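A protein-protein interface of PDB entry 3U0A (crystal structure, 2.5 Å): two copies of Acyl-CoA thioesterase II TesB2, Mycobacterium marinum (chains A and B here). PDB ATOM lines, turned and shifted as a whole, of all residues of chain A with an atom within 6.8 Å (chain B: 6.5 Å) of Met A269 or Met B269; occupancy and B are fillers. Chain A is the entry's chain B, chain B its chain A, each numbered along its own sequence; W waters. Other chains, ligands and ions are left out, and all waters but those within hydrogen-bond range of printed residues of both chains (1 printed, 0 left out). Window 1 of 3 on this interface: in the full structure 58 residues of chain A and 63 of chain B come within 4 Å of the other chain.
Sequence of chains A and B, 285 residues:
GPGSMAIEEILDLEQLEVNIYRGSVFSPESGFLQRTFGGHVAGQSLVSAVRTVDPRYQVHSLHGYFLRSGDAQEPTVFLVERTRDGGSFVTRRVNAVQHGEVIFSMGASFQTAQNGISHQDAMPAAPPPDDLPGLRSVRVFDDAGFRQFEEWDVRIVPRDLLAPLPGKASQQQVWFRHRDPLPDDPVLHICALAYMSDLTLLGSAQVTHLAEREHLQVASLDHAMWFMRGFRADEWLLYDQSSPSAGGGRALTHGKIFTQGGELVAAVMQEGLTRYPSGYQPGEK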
ATOM      1  N   HIS A  63     -21.405 -26.603  23.680  1.00  0.00           N
ATOM      2  CA  HIS A  63     -22.051 -25.557  22.883  1.00  0.00           C
ATOM      3  C   HIS A  63     -21.660 -24.205  23.426  1.00  0.00           C
ATOM      4  O   HIS A  63     -21.639 -24.001  24.620  1.00  0.00           O
ATOM      5  CB  HIS A  63     -23.587 -25.589  22.862  1.00  0.00           C
ATOM      6  CG  HIS A  63     -24.241 -26.964  22.726  1.00  0.00           C
ATOM      7  ND1 HIS A  63     -25.267 -27.363  23.546  1.00  0.00           N
ATOM      8  CD2 HIS A  63     -24.059 -27.999  21.799  1.00  0.00           C
ATOM      9  CE1 HIS A  63     -25.665 -28.613  23.185  1.00  0.00           C
ATOM     10  NE2 HIS A  63     -24.917 -29.008  22.124  1.00  0.00           N
ATOM     11  N   LEU A 201     -12.914 -23.659   9.630  1.00  0.00           N
ATOM     12  CA  LEU A 201     -14.286 -24.072   9.345  1.00  0.00           C
ATOM     13  C   LEU A 201     -15.145 -23.007   8.676  1.00  0.00           C
ATOM     14  O   LEU A 201     -15.765 -23.268   7.659  1.00  0.00           O
ATOM     15  CB  LEU A 201     -14.987 -24.495  10.631  1.00  0.00           C
ATOM     16  CG  LEU A 201     -15.983 -25.650  10.552  1.00  0.00           C
ATOM     17  CD1 LEU A 201     -17.113 -25.349  11.503  1.00  0.00           C
ATOM     18  CD2 LEU A 201     -16.490 -26.003   9.157  1.00  0.00           C
ATOM     19  N   ASP A 222     -21.120 -18.901  16.919  1.00  0.00           N
ATOM     20  CA  ASP A 222     -21.359 -20.018  17.829  1.00  0.00           C
ATOM     21  C   ASP A 222     -20.448 -21.193  17.562  1.00  0.00           C
ATOM     22  O   ASP A 222     -19.697 -21.200  16.602  1.00  0.00           O
ATOM     23  CB  ASP A 222     -22.882 -20.391  17.907  1.00  0.00           C
ATOM     24  CG  ASP A 222     -23.407 -21.140  16.696  1.00  0.00           C
ATOM     25  OD1 ASP A 222     -22.597 -21.647  15.920  1.00  0.00           O
ATOM     26  OD2 ASP A 222     -24.651 -21.265  16.546  1.00  0.00           O
ATOM     27  N   HIS A 223     -20.495 -22.167  18.456  1.00  0.00           N
ATOM     28  CA  HIS A 223     -19.729 -23.373  18.298  1.00  0.00           C
ATOM     29  C   HIS A 223     -20.389 -24.559  18.957  1.00  0.00           C
ATOM     30  O   HIS A 223     -20.878 -24.460  20.074  1.00  0.00           O
ATOM     31  CB  HIS A 223     -18.360 -23.159  18.885  1.00  0.00           C
ATOM     32  CG  HIS A 223     -17.279 -23.890  18.159  1.00  0.00           C
ATOM     33  ND1 HIS A 223     -17.011 -23.671  16.858  1.00  0.00           N
ATOM     34  CD2 HIS A 223     -16.366 -24.838  18.599  1.00  0.00           C
ATOM     35  CE1 HIS A 223     -15.973 -24.440  16.467  1.00  0.00           C
ATOM     36  NE2 HIS A 223     -15.581 -25.175  17.532  1.00  0.00           N
ATOM     37  N   ALA A 224     -20.431 -25.685  18.267  1.00  0.00           N
ATOM     38  CA  ALA A 224     -20.981 -26.892  18.831  1.00  0.00           C
ATOM     39  C   ALA A 224     -20.134 -28.076  18.368  1.00  0.00           C
ATOM     40  O   ALA A 224     -19.860 -28.240  17.177  1.00  0.00           O
ATOM     41  CB  ALA A 224     -22.419 -27.052  18.425  1.00  0.00           C
ATOM     42  N   MET A 225     -19.717 -28.894  19.328  1.00  0.00           N
ATOM     43  CA  MET A 225     -18.775 -29.972  19.047  1.00  0.00           C
ATOM     44  C   MET A 225     -19.115 -31.235  19.756  1.00  0.00           C
ATOM     45  O   MET A 225     -19.469 -31.202  20.886  1.00  0.00           O
ATOM     46  CB  MET A 225     -17.355 -29.590  19.475  1.00  0.00           C
ATOM     47  CG  MET A 225     -16.569 -28.852  18.424  1.00  0.00           C
ATOM     48  SD  MET A 225     -14.839 -28.619  18.875  1.00  0.00           S
ATOM     49  CE  MET A 225     -14.206 -30.272  18.482  1.00  0.00           C
ATOM     50  N   TRP A 226     -18.917 -32.348  19.082  1.00  0.00           N
ATOM     51  CA  TRP A 226     -19.185 -33.654  19.622  1.00  0.00           C
ATOM     52  C   TRP A 226     -17.935 -34.527  19.519  1.00  0.00           C
ATOM     53  O   TRP A 226     -17.391 -34.730  18.437  1.00  0.00           O
ATOM     54  CB  TRP A 226     -20.382 -34.263  18.909  1.00  0.00           C
ATOM     55  CG  TRP A 226     -21.663 -33.503  19.155  1.00  0.00           C
ATOM     56  CD1 TRP A 226     -22.629 -33.759  20.116  1.00  0.00           C
ATOM     57  CD2 TRP A 226     -22.148 -32.322  18.440  1.00  0.00           C
ATOM     58  NE1 TRP A 226     -23.627 -32.847  20.051  1.00  0.00           N
ATOM     59  CE2 TRP A 226     -23.399 -31.957  19.068  1.00  0.00           C
ATOM     60  CE3 TRP A 226     -21.670 -31.553  17.396  1.00  0.00           C
ATOM     61  CZ2 TRP A 226     -24.145 -30.867  18.634  1.00  0.00           C
ATOM     62  CZ3 TRP A 226     -22.412 -30.457  16.971  1.00  0.00           C
ATOM     63  CH2 TRP A 226     -23.625 -30.124  17.570  1.00  0.00           C
ATOM     64  N   TYR A 239     -10.095 -32.648   8.144  1.00  0.00           N
ATOM     65  CA  TYR A 239     -11.213 -31.874   8.510  1.00  0.00           C
ATOM     66  C   TYR A 239     -12.024 -31.665   7.254  1.00  0.00           C
ATOM     67  O   TYR A 239     -11.716 -30.781   6.474  1.00  0.00           O
ATOM     68  CB  TYR A 239     -10.739 -30.544   9.044  1.00  0.00           C
ATOM     69  CG  TYR A 239     -11.686 -29.833   9.999  1.00  0.00           C
ATOM     70  CD1 TYR A 239     -12.928 -30.340  10.331  1.00  0.00           C
ATOM     71  CD2 TYR A 239     -11.301 -28.643  10.581  1.00  0.00           C
ATOM     72  CE1 TYR A 239     -13.754 -29.682  11.236  1.00  0.00           C
ATOM     73  CE2 TYR A 239     -12.105 -27.971  11.475  1.00  0.00           C
ATOM     74  CZ  TYR A 239     -13.339 -28.484  11.803  1.00  0.00           C
ATOM     75  OH  TYR A 239     -14.130 -27.767  12.691  1.00  0.00           O
ATOM     76  N   PRO A 244     -23.779 -25.697   4.371  1.00  0.00           N
ATOM     77  CA  PRO A 244     -25.009 -25.998   3.624  1.00  0.00           C
ATOM     78  C   PRO A 244     -25.922 -24.822   3.372  1.00  0.00           C
ATOM     79  O   PRO A 244     -26.848 -24.960   2.623  1.00  0.00           O
ATOM     80  CB  PRO A 244     -25.713 -27.006   4.532  1.00  0.00           C
ATOM     81  CG  PRO A 244     -25.248 -26.655   5.887  1.00  0.00           C
ATOM     82  CD  PRO A 244     -23.814 -26.256   5.723  1.00  0.00           C
ATOM     83  N   LEU A 252     -23.919 -21.088   7.838  1.00  0.00           N
ATOM     84  CA  LEU A 252     -23.762 -22.247   8.665  1.00  0.00           C
ATOM     85  C   LEU A 252     -22.687 -23.123   8.066  1.00  0.00           C
ATOM     86  O   LEU A 252     -22.633 -23.295   6.871  1.00  0.00           O
ATOM     87  CB  LEU A 252     -25.071 -23.023   8.727  1.00  0.00           C
ATOM     88  CG  LEU A 252     -25.117 -24.144   9.774  1.00  0.00           C
ATOM     89  CD1 LEU A 252     -24.894 -23.671  11.213  1.00  0.00           C
ATOM     90  CD2 LEU A 252     -26.464 -24.845   9.657  1.00  0.00           C
ATOM     91  N   THR A 253     -21.823 -23.656   8.908  1.00  0.00           N
ATOM     92  CA  THR A 253     -20.792 -24.585   8.480  1.00  0.00           C
ATOM     93  C   THR A 253     -20.835 -25.827   9.335  1.00  0.00           C
ATOM     94  O   THR A 253     -21.353 -25.814  10.464  1.00  0.00           O
ATOM     95  CB  THR A 253     -19.420 -23.950   8.578  1.00  0.00           C
ATOM     96  OG1 THR A 253     -19.155 -23.611   9.932  1.00  0.00           O
ATOM     97  CG2 THR A 253     -19.382 -22.707   7.740  1.00  0.00           C
ATOM     98  N   HIS A 254     -20.286 -26.898   8.797  1.00  0.00           N
ATOM     99  CA  HIS A 254     -20.408 -28.227   9.362  1.00  0.00           C
ATOM    100  C   HIS A 254     -19.131 -28.942   9.065  1.00  0.00           C
ATOM    101  O   HIS A 254     -18.699 -28.949   7.916  1.00  0.00           O
ATOM    102  CB  HIS A 254     -21.560 -28.919   8.662  1.00  0.00           C
ATOM    103  CG  HIS A 254     -21.863 -30.311   9.168  1.00  0.00           C
ATOM    104  ND1 HIS A 254     -22.815 -31.086   8.613  1.00  0.00           N
ATOM    105  CD2 HIS A 254     -21.320 -31.059  10.222  1.00  0.00           C
ATOM    106  CE1 HIS A 254     -22.883 -32.264   9.296  1.00  0.00           C
ATOM    107  NE2 HIS A 254     -21.963 -32.247  10.263  1.00  0.00           N
ATOM    108  N   GLY A 255     -18.517 -29.565  10.068  1.00  0.00           N
ATOM    109  CA  GLY A 255     -17.272 -30.318   9.860  1.00  0.00           C
ATOM    110  C   GLY A 255     -17.246 -31.717  10.426  1.00  0.00           C
ATOM    111  O   GLY A 255     -17.922 -32.009  11.371  1.00  0.00           O
ATOM    112  N   ALA A 267     -17.360 -34.202  15.538  1.00  0.00           N
ATOM    113  CA  ALA A 267     -18.199 -33.473  14.607  1.00  0.00           C
ATOM    114  C   ALA A 267     -18.330 -32.053  15.110  1.00  0.00           C
ATOM    115  O   ALA A 267     -18.344 -31.810  16.304  1.00  0.00           O
ATOM    116  CB  ALA A 267     -19.565 -34.127  14.492  1.00  0.00           C
ATOM    117  N   VAL A 268     -18.410 -31.114  14.188  1.00  0.00           N
ATOM    118  CA  VAL A 268     -18.489 -29.722  14.550  1.00  0.00           C
ATOM    119  C   VAL A 268     -19.576 -29.018  13.756  1.00  0.00           C
ATOM    120  O   VAL A 268     -19.767 -29.309  12.595  1.00  0.00           O
ATOM    121  CB  VAL A 268     -17.144 -28.985  14.317  1.00  0.00           C
ATOM    122  CG1 VAL A 268     -17.177 -27.607  14.955  1.00  0.00           C
ATOM    123  CG2 VAL A 268     -15.959 -29.788  14.824  1.00  0.00           C
ATOM    124  N   MET A 269     -20.292 -28.093  14.403  1.00  0.00           N
ATOM    125  CA  MET A 269     -21.144 -27.118  13.707  1.00  0.00           C
ATOM    126  C   MET A 269     -20.825 -25.685  14.101  1.00  0.00           C
ATOM    127  O   MET A 269     -20.620 -25.424  15.244  1.00  0.00           O
ATOM    128  CB  MET A 269     -22.594 -27.397  13.998  1.00  0.00           C
ATOM    129  CG  MET A 269     -23.089 -28.593  13.239  1.00  0.00           C
ATOM    130  SD  MET A 269     -23.416 -28.159  11.539  1.00  0.00           S
ATOM    131  CE  MET A 269     -25.214 -28.230  11.527  1.00  0.00           C
ATOM    132  N   GLN A 270     -20.812 -24.766  13.150  1.00  0.00           N
ATOM    133  CA  GLN A 270     -20.506 -23.374  13.449  1.00  0.00           C
ATOM    134  C   GLN A 270     -21.239 -22.386  12.538  1.00  0.00           C
ATOM    135  O   GLN A 270     -21.125 -22.455  11.332  1.00  0.00           O
ATOM    136  CB  GLN A 270     -19.006 -23.152  13.338  1.00  0.00           C
ATOM    137  CG  GLN A 270     -18.596 -21.723  13.600  1.00  0.00           C
ATOM    138  CD  GLN A 270     -17.119 -21.602  13.901  1.00  0.00           C
ATOM    139  OE1 GLN A 270     -16.264 -21.989  13.074  1.00  0.00           O
ATOM    140  NE2 GLN A 270     -16.797 -21.092  15.081  1.00  0.00           N
ATOM    141  N   GLU A 271     -22.019 -21.496  13.143  1.00  0.00           N
ATOM    142  CA  GLU A 271     -22.661 -20.413  12.450  1.00  0.00           C
ATOM    143  C   GLU A 271     -21.737 -19.187  12.559  1.00  0.00           C
ATOM    144  O   GLU A 271     -21.027 -19.026  13.524  1.00  0.00           O
ATOM    145  CB  GLU A 271     -24.082 -20.130  12.996  1.00  0.00           C
ATOM    146  CG  GLU A 271     -24.896 -19.239  12.047  1.00  0.00           C
ATOM    147  CD  GLU A 271     -26.355 -19.040  12.413  1.00  0.00           C
ATOM    148  OE1 GLU A 271     -26.710 -18.931  13.599  1.00  0.00           O
ATOM    149  OE2 GLU A 271     -27.149 -18.941  11.484  1.00  0.00           O
ATOM    150  N   HIS B  63     -29.292 -23.816  21.396  1.00  0.00           N
ATOM    151  CA  HIS B  63     -28.543 -24.977  21.835  1.00  0.00           C
ATOM    152  C   HIS B  63     -29.092 -25.259  23.206  1.00  0.00           C
ATOM    153  O   HIS B  63     -29.302 -24.356  23.960  1.00  0.00           O
ATOM    154  CB  HIS B  63     -27.042 -24.701  21.948  1.00  0.00           C
ATOM    155  CG  HIS B  63     -26.364 -24.084  20.700  1.00  0.00           C
ATOM    156  ND1 HIS B  63     -26.502 -22.780  20.355  1.00  0.00           N
ATOM    157  CD2 HIS B  63     -25.433 -24.627  19.775  1.00  0.00           C
ATOM    158  CE1 HIS B  63     -25.768 -22.515  19.233  1.00  0.00           C
ATOM    159  NE2 HIS B  63     -25.101 -23.638  18.891  1.00  0.00           N
ATOM    160  N   LEU B 201     -35.988 -37.040  15.329  1.00  0.00           N
ATOM    161  CA  LEU B 201     -34.611 -37.204  14.821  1.00  0.00           C
ATOM    162  C   LEU B 201     -33.830 -38.361  15.409  1.00  0.00           C
ATOM    163  O   LEU B 201     -33.228 -39.076  14.670  1.00  0.00           O
ATOM    164  CB  LEU B 201     -33.778 -35.940  14.970  1.00  0.00           C
ATOM    165  CG  LEU B 201     -32.389 -35.934  14.336  1.00  0.00           C
ATOM    166  CD1 LEU B 201     -32.427 -36.180  12.837  1.00  0.00           C
ATOM    167  CD2 LEU B 201     -31.762 -34.580  14.622  1.00  0.00           C
ATOM    168  N   ASP B 222     -29.121 -33.635  24.228  1.00  0.00           N
ATOM    169  CA  ASP B 222     -29.081 -32.260  23.802  1.00  0.00           C
ATOM    170  C   ASP B 222     -29.874 -32.005  22.531  1.00  0.00           C
ATOM    171  O   ASP B 222     -30.592 -32.875  22.066  1.00  0.00           O
ATOM    172  CB  ASP B 222     -27.619 -31.784  23.682  1.00  0.00           C
ATOM    173  CG  ASP B 222     -26.912 -32.250  22.413  1.00  0.00           C
ATOM    174  OD1 ASP B 222     -27.544 -32.652  21.418  1.00  0.00           O
ATOM    175  OD2 ASP B 222     -25.680 -32.146  22.425  1.00  0.00           O
ATOM    176  N   HIS B 223     -29.823 -30.765  22.068  1.00  0.00           N
ATOM    177  CA  HIS B 223     -30.129 -30.423  20.709  1.00  0.00           C
ATOM    178  C   HIS B 223     -29.535 -29.060  20.400  1.00  0.00           C
ATOM    179  O   HIS B 223     -29.296 -28.238  21.295  1.00  0.00           O
ATOM    180  CB  HIS B 223     -31.646 -30.530  20.364  1.00  0.00           C
ATOM    181  CG  HIS B 223     -32.547 -29.498  21.042  1.00  0.00           C
ATOM    182  ND1 HIS B 223     -33.862 -29.624  21.054  1.00  0.00           N
ATOM    183  CD2 HIS B 223     -32.265 -28.310  21.713  1.00  0.00           C
ATOM    184  CE1 HIS B 223     -34.409 -28.560  21.697  1.00  0.00           C
ATOM    185  NE2 HIS B 223     -33.428 -27.776  22.102  1.00  0.00           N
ATOM    186  N   ALA B 224     -29.266 -28.863  19.114  1.00  0.00           N
ATOM    187  CA  ALA B 224     -28.727 -27.626  18.557  1.00  0.00           C
ATOM    188  C   ALA B 224     -29.473 -27.422  17.271  1.00  0.00           C
ATOM    189  O   ALA B 224     -29.586 -28.360  16.487  1.00  0.00           O
ATOM    190  CB  ALA B 224     -27.221 -27.756  18.280  1.00  0.00           C
ATOM    191  N   MET B 225     -29.983 -26.209  17.053  1.00  0.00           N
ATOM    192  CA  MET B 225     -30.806 -25.903  15.855  1.00  0.00           C
ATOM    193  C   MET B 225     -30.475 -24.550  15.248  1.00  0.00           C
ATOM    194  O   MET B 225     -30.023 -23.635  15.943  1.00  0.00           O
ATOM    195  CB  MET B 225     -32.287 -25.939  16.189  1.00  0.00           C
ATOM    196  CG  MET B 225     -32.766 -27.267  16.745  1.00  0.00           C
ATOM    197  SD  MET B 225     -34.508 -27.262  17.165  1.00  0.00           S
ATOM    198  CE  MET B 225     -34.616 -28.890  17.957  1.00  0.00           C
ATOM    199  N   TRP B 226     -30.689 -24.442  13.933  1.00  0.00           N
ATOM    200  CA  TRP B 226     -30.421 -23.212  13.211  1.00  0.00           C
ATOM    201  C   TRP B 226     -31.550 -22.960  12.295  1.00  0.00           C
ATOM    202  O   TRP B 226     -31.854 -23.790  11.464  1.00  0.00           O
ATOM    203  CB  TRP B 226     -29.096 -23.314  12.452  1.00  0.00           C
ATOM    204  CG  TRP B 226     -27.879 -23.488  13.364  1.00  0.00           C
ATOM    205  CD1 TRP B 226     -27.060 -22.507  13.885  1.00  0.00           C
ATOM    206  CD2 TRP B 226     -27.319 -24.725  13.861  1.00  0.00           C
ATOM    207  NE1 TRP B 226     -26.071 -23.037  14.653  1.00  0.00           N
ATOM    208  CE2 TRP B 226     -26.183 -24.358  14.697  1.00  0.00           C
ATOM    209  CE3 TRP B 226     -27.633 -26.059  13.712  1.00  0.00           C
ATOM    210  CZ2 TRP B 226     -25.409 -25.304  15.331  1.00  0.00           C
ATOM    211  CZ3 TRP B 226     -26.840 -27.011  14.372  1.00  0.00           C
ATOM    212  CH2 TRP B 226     -25.751 -26.632  15.152  1.00  0.00           C
ATOM    213  N   TYR B 239     -37.827 -33.929   6.162  1.00  0.00           N
ATOM    214  CA  TYR B 239     -36.762 -34.051   7.083  1.00  0.00           C
ATOM    215  C   TYR B 239     -35.765 -35.051   6.563  1.00  0.00           C
ATOM    216  O   TYR B 239     -36.004 -36.246   6.586  1.00  0.00           O
ATOM    217  CB  TYR B 239     -37.250 -34.547   8.413  1.00  0.00           C
ATOM    218  CG  TYR B 239     -36.426 -34.035   9.550  1.00  0.00           C
ATOM    219  CD1 TYR B 239     -35.173 -33.422   9.356  1.00  0.00           C
ATOM    220  CD2 TYR B 239     -36.886 -34.167  10.843  1.00  0.00           C
ATOM    221  CE1 TYR B 239     -34.436 -32.935  10.447  1.00  0.00           C
ATOM    222  CE2 TYR B 239     -36.156 -33.691  11.933  1.00  0.00           C
ATOM    223  CZ  TYR B 239     -34.958 -33.064  11.755  1.00  0.00           C
ATOM    224  OH  TYR B 239     -34.338 -32.596  12.902  1.00  0.00           O
ATOM    225  N   PRO B 244     -24.557 -40.085  11.862  1.00  0.00           N
ATOM    226  CA  PRO B 244     -23.225 -40.356  11.355  1.00  0.00           C
ATOM    227  C   PRO B 244     -22.414 -41.254  12.275  1.00  0.00           C
ATOM    228  O   PRO B 244     -21.406 -41.796  11.851  1.00  0.00           O
ATOM    229  CB  PRO B 244     -22.608 -38.971  11.233  1.00  0.00           C
ATOM    230  CG  PRO B 244     -23.353 -38.128  12.177  1.00  0.00           C
ATOM    231  CD  PRO B 244     -24.735 -38.668  12.232  1.00  0.00           C
ATOM    232  N   LEU B 252     -25.075 -39.883  17.739  1.00  0.00           N
ATOM    233  CA  LEU B 252     -25.237 -38.569  17.231  1.00  0.00           C
ATOM    234  C   LEU B 252     -26.113 -38.652  16.021  1.00  0.00           C
ATOM    235  O   LEU B 252     -26.005 -39.583  15.224  1.00  0.00           O
ATOM    236  CB  LEU B 252     -23.897 -37.992  16.841  1.00  0.00           C
ATOM    237  CG  LEU B 252     -23.881 -36.508  16.521  1.00  0.00           C
ATOM    238  CD1 LEU B 252     -24.349 -35.712  17.741  1.00  0.00           C
ATOM    239  CD2 LEU B 252     -22.485 -36.121  16.065  1.00  0.00           C
ATOM    240  N   THR B 253     -26.992 -37.663  15.897  1.00  0.00           N
ATOM    241  CA  THR B 253     -27.861 -37.526  14.744  1.00  0.00           C
ATOM    242  C   THR B 253     -27.886 -36.072  14.249  1.00  0.00           C
ATOM    243  O   THR B 253     -27.417 -35.135  14.894  1.00  0.00           O
ATOM    244  CB  THR B 253     -29.273 -38.075  15.052  1.00  0.00           C
ATOM    245  OG1 THR B 253     -29.933 -37.266  16.040  1.00  0.00           O
ATOM    246  CG2 THR B 253     -29.177 -39.537  15.542  1.00  0.00           C
ATOM    247  N   HIS B 254     -28.424 -35.920  13.055  1.00  0.00           N
ATOM    248  CA  HIS B 254     -28.236 -34.715  12.264  1.00  0.00           C
ATOM    249  C   HIS B 254     -29.276 -34.643  11.204  1.00  0.00           C
ATOM    250  O   HIS B 254     -29.543 -35.660  10.527  1.00  0.00           O
ATOM    251  CB  HIS B 254     -26.882 -34.762  11.578  1.00  0.00           C
ATOM    252  CG  HIS B 254     -26.689 -33.667  10.569  1.00  0.00           C
ATOM    253  ND1 HIS B 254     -26.444 -32.403  10.924  1.00  0.00           N
ATOM    254  CD2 HIS B 254     -26.768 -33.681   9.168  1.00  0.00           C
ATOM    255  CE1 HIS B 254     -26.338 -31.638   9.814  1.00  0.00           C
ATOM    256  NE2 HIS B 254     -26.541 -32.424   8.743  1.00  0.00           N
ATOM    257  N   GLY B 255     -29.843 -33.458  10.989  1.00  0.00           N
ATOM    258  CA  GLY B 255     -30.720 -33.318   9.856  1.00  0.00           C
ATOM    259  C   GLY B 255     -30.928 -31.939   9.305  1.00  0.00           C
ATOM    260  O   GLY B 255     -30.583 -30.961   9.952  1.00  0.00           O
ATOM    261  N   ALA B 267     -31.555 -26.615  10.085  1.00  0.00           N
ATOM    262  CA  ALA B 267     -30.566 -27.661  10.316  1.00  0.00           C
ATOM    263  C   ALA B 267     -30.616 -28.022  11.773  1.00  0.00           C
ATOM    264  O   ALA B 267     -30.890 -27.167  12.608  1.00  0.00           O
ATOM    265  CB  ALA B 267     -29.171 -27.200   9.948  1.00  0.00           C
ATOM    266  N   VAL B 268     -30.408 -29.294  12.089  1.00  0.00           N
ATOM    267  CA  VAL B 268     -30.433 -29.739  13.478  1.00  0.00           C
ATOM    268  C   VAL B 268     -29.352 -30.773  13.708  1.00  0.00           C
ATOM    269  O   VAL B 268     -29.124 -31.626  12.859  1.00  0.00           O
ATOM    270  CB  VAL B 268     -31.776 -30.409  13.875  1.00  0.00           C
ATOM    271  CG1 VAL B 268     -31.728 -30.886  15.313  1.00  0.00           C
ATOM    272  CG2 VAL B 268     -32.972 -29.479  13.663  1.00  0.00           C
ATOM    273  N   MET B 269     -28.696 -30.690  14.862  1.00  0.00           N
ATOM    274  CA  MET B 269     -27.877 -31.780  15.392  1.00  0.00           C
ATOM    275  C   MET B 269     -28.352 -32.110  16.791  1.00  0.00           C
ATOM    276  O   MET B 269     -28.663 -31.207  17.546  1.00  0.00           O
ATOM    277  CB  MET B 269     -26.447 -31.346  15.460  1.00  0.00           C
ATOM    278  CG  MET B 269     -25.790 -31.333  14.106  1.00  0.00           C
ATOM    279  SD  MET B 269     -25.030 -32.938  13.940  1.00  0.00           S
ATOM    280  CE  MET B 269     -23.314 -32.531  14.214  1.00  0.00           C
ATOM    281  N   GLN B 270     -28.388 -33.401  17.125  1.00  0.00           N
ATOM    282  CA  GLN B 270     -28.832 -33.877  18.417  1.00  0.00           C
ATOM    283  C   GLN B 270     -28.131 -35.162  18.776  1.00  0.00           C
ATOM    284  O   GLN B 270     -28.014 -36.084  17.960  1.00  0.00           O
ATOM    285  CB  GLN B 270     -30.334 -34.097  18.388  1.00  0.00           C
ATOM    286  CG  GLN B 270     -30.975 -34.690  19.628  1.00  0.00           C
ATOM    287  CD  GLN B 270     -32.486 -34.451  19.649  1.00  0.00           C
ATOM    288  OE1 GLN B 270     -33.142 -34.595  18.617  1.00  0.00           O
ATOM    289  NE2 GLN B 270     -33.037 -34.066  20.798  1.00  0.00           N
ATOM    290  N   GLU B 271     -27.642 -35.197  20.009  1.00  0.00           N
ATOM    291  CA  GLU B 271     -27.048 -36.395  20.564  1.00  0.00           C
ATOM    292  C   GLU B 271     -28.058 -37.033  21.558  1.00  0.00           C
ATOM    293  O   GLU B 271     -28.793 -36.324  22.243  1.00  0.00           O
ATOM    294  CB  GLU B 271     -25.723 -36.050  21.234  1.00  0.00           C
ATOM    295  CG  GLU B 271     -24.947 -37.270  21.686  1.00  0.00           C
ATOM    296  CD  GLU B 271     -23.539 -36.942  22.166  1.00  0.00           C
ATOM    297  OE1 GLU B 271     -23.366 -35.987  23.003  1.00  0.00           O
ATOM    298  OE2 GLU B 271     -22.610 -37.663  21.701  1.00  0.00           O
HETATM  299  O   HOH W   1     -23.020 -24.330  16.580  1.00  0.00           O
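NE2 of His B63 lies close to OD2 of Asp A222 (3.4 Å).
NE2 of His A63 is in hydrogen-bond range of OD2 of Asp B222 (3.2 Å).
NE1 of Trp A226 sits at hydrogen-bond distance from OD2 of Asp B222, 3.2 Å away.
NE1 of Trp B226 lies within hydrogen-bond range of OD2 of Asp A222.
The side-chain amide nitrogen of Gln B270 lies within hydrogen-bond range of the backbone carbonyl oxygen of Asp B222 (3.0 Å).
The backbone NH (N) of Glu B271 lies within hydrogen-bond range of the side-chain carboxylate (OD1) of Asp B222, at 2.9 Å.
The backbone carbonyl oxygen of Met B269 sits at hydrogen-bond distance from the backbone NH of Ala B224 (2.9 Å).
N of Trp B226 lies within hydrogen-bond range of O of Ala B267 (3.0 Å).
NE2 of Gln A270 lies close to O of Asp A222 (3.3 Å).
His A63 touches His B63 (ND1 to CB, 3.6 Å).
Leu B252 touches Trp A226 (CD1 to CD1, 3.5 Å).
CD1 of Trp A226 touches OE1 of Glu B271, 3.7 Å away.
Leu A252 touches Trp B226.
Ala B267 touches Leu A252 (CB to CD2, 3.6 Å).
CE1 of His A254 touches CE1 of His B254, at 3.5 Å.
CD2 of Leu B252 touches CB of Ala A267 (3.9 Å).
Trp B226 touches Met A269.
Met A269 touches His B254.
CD1 of Trp B226 touches OE1 of Glu A271, 3.6 Å away.
Of the printed residues of chain B, Asp A222 touches His B63 and Trp B226.
Of the printed residues of chain B, Ala A267 touches Leu B252 (3.9 Å).
Of the printed residues of chain A, His B254 touches His A254 and Met A269.
Gln B270 touches none of the printed residues of chain A.
The nearest residue of chain B that does not touch Met A269 is Ala B267 (4.4 Å).
The nearest residue of chain A that does not touch Met B269 is Ala A267 (4.1 Å).
The nearest printed residue of chain B that does not touch Ala A267 is Met B269 (4.1 Å).
Of the 18 printed residues of chain A, 8 touch a printed residue of chain B.
Printed residues of chain A that touch a printed residue of chain B: His A63, Asp A222, Trp A226, Leu A252, His A254, Ala A267, Met A269 and Glu A271.
Hydrophobic or aromatic side chains of chain A within 4 Å of the printed part of chain B: His A63, Trp A226, Leu A252, His A254, Ala A267 and Met A269.
Of the 18 printed residues of chain B, 8 touch a printed residue of chain A.
Printed residues of chain B that touch a printed residue of chain A: His B63, Asp B222, Trp B226, Leu B252, His B254, Ala B267, Met B269 and Glu B271.
Hydrophobic or aromatic side chains of chain B within 4 Å of the printed part of chain A: His B63, Trp B226, Leu B252, His B254, Ala B267 and Met B269.
Among the printed residues, no Asp or Glu carboxylate lies within 4 Å of a Lys or Arg side-chain nitrogen of the other chain.
His B63 touches its own counterpart, His A63.
His A63 touches Asp B222, and with the chains exchanged Asp A222 touches His B63.
Leu A252 touches Ala B267, and with the chains exchanged Ala A267 touches Leu B252.
His B254 touches its own counterpart, His A254.
Of the 16 pairs that touch across the chains among the printed residues, 15 have their exchanged pair printed and touching as well.
Water W1 lies within hydrogen-bond range of OD1 of Asp A222 (2.8 Å), O of Met A269 (3.0 Å), NE2 of His B63 (3.2 Å) and N of Ala A224 (3.4 Å).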
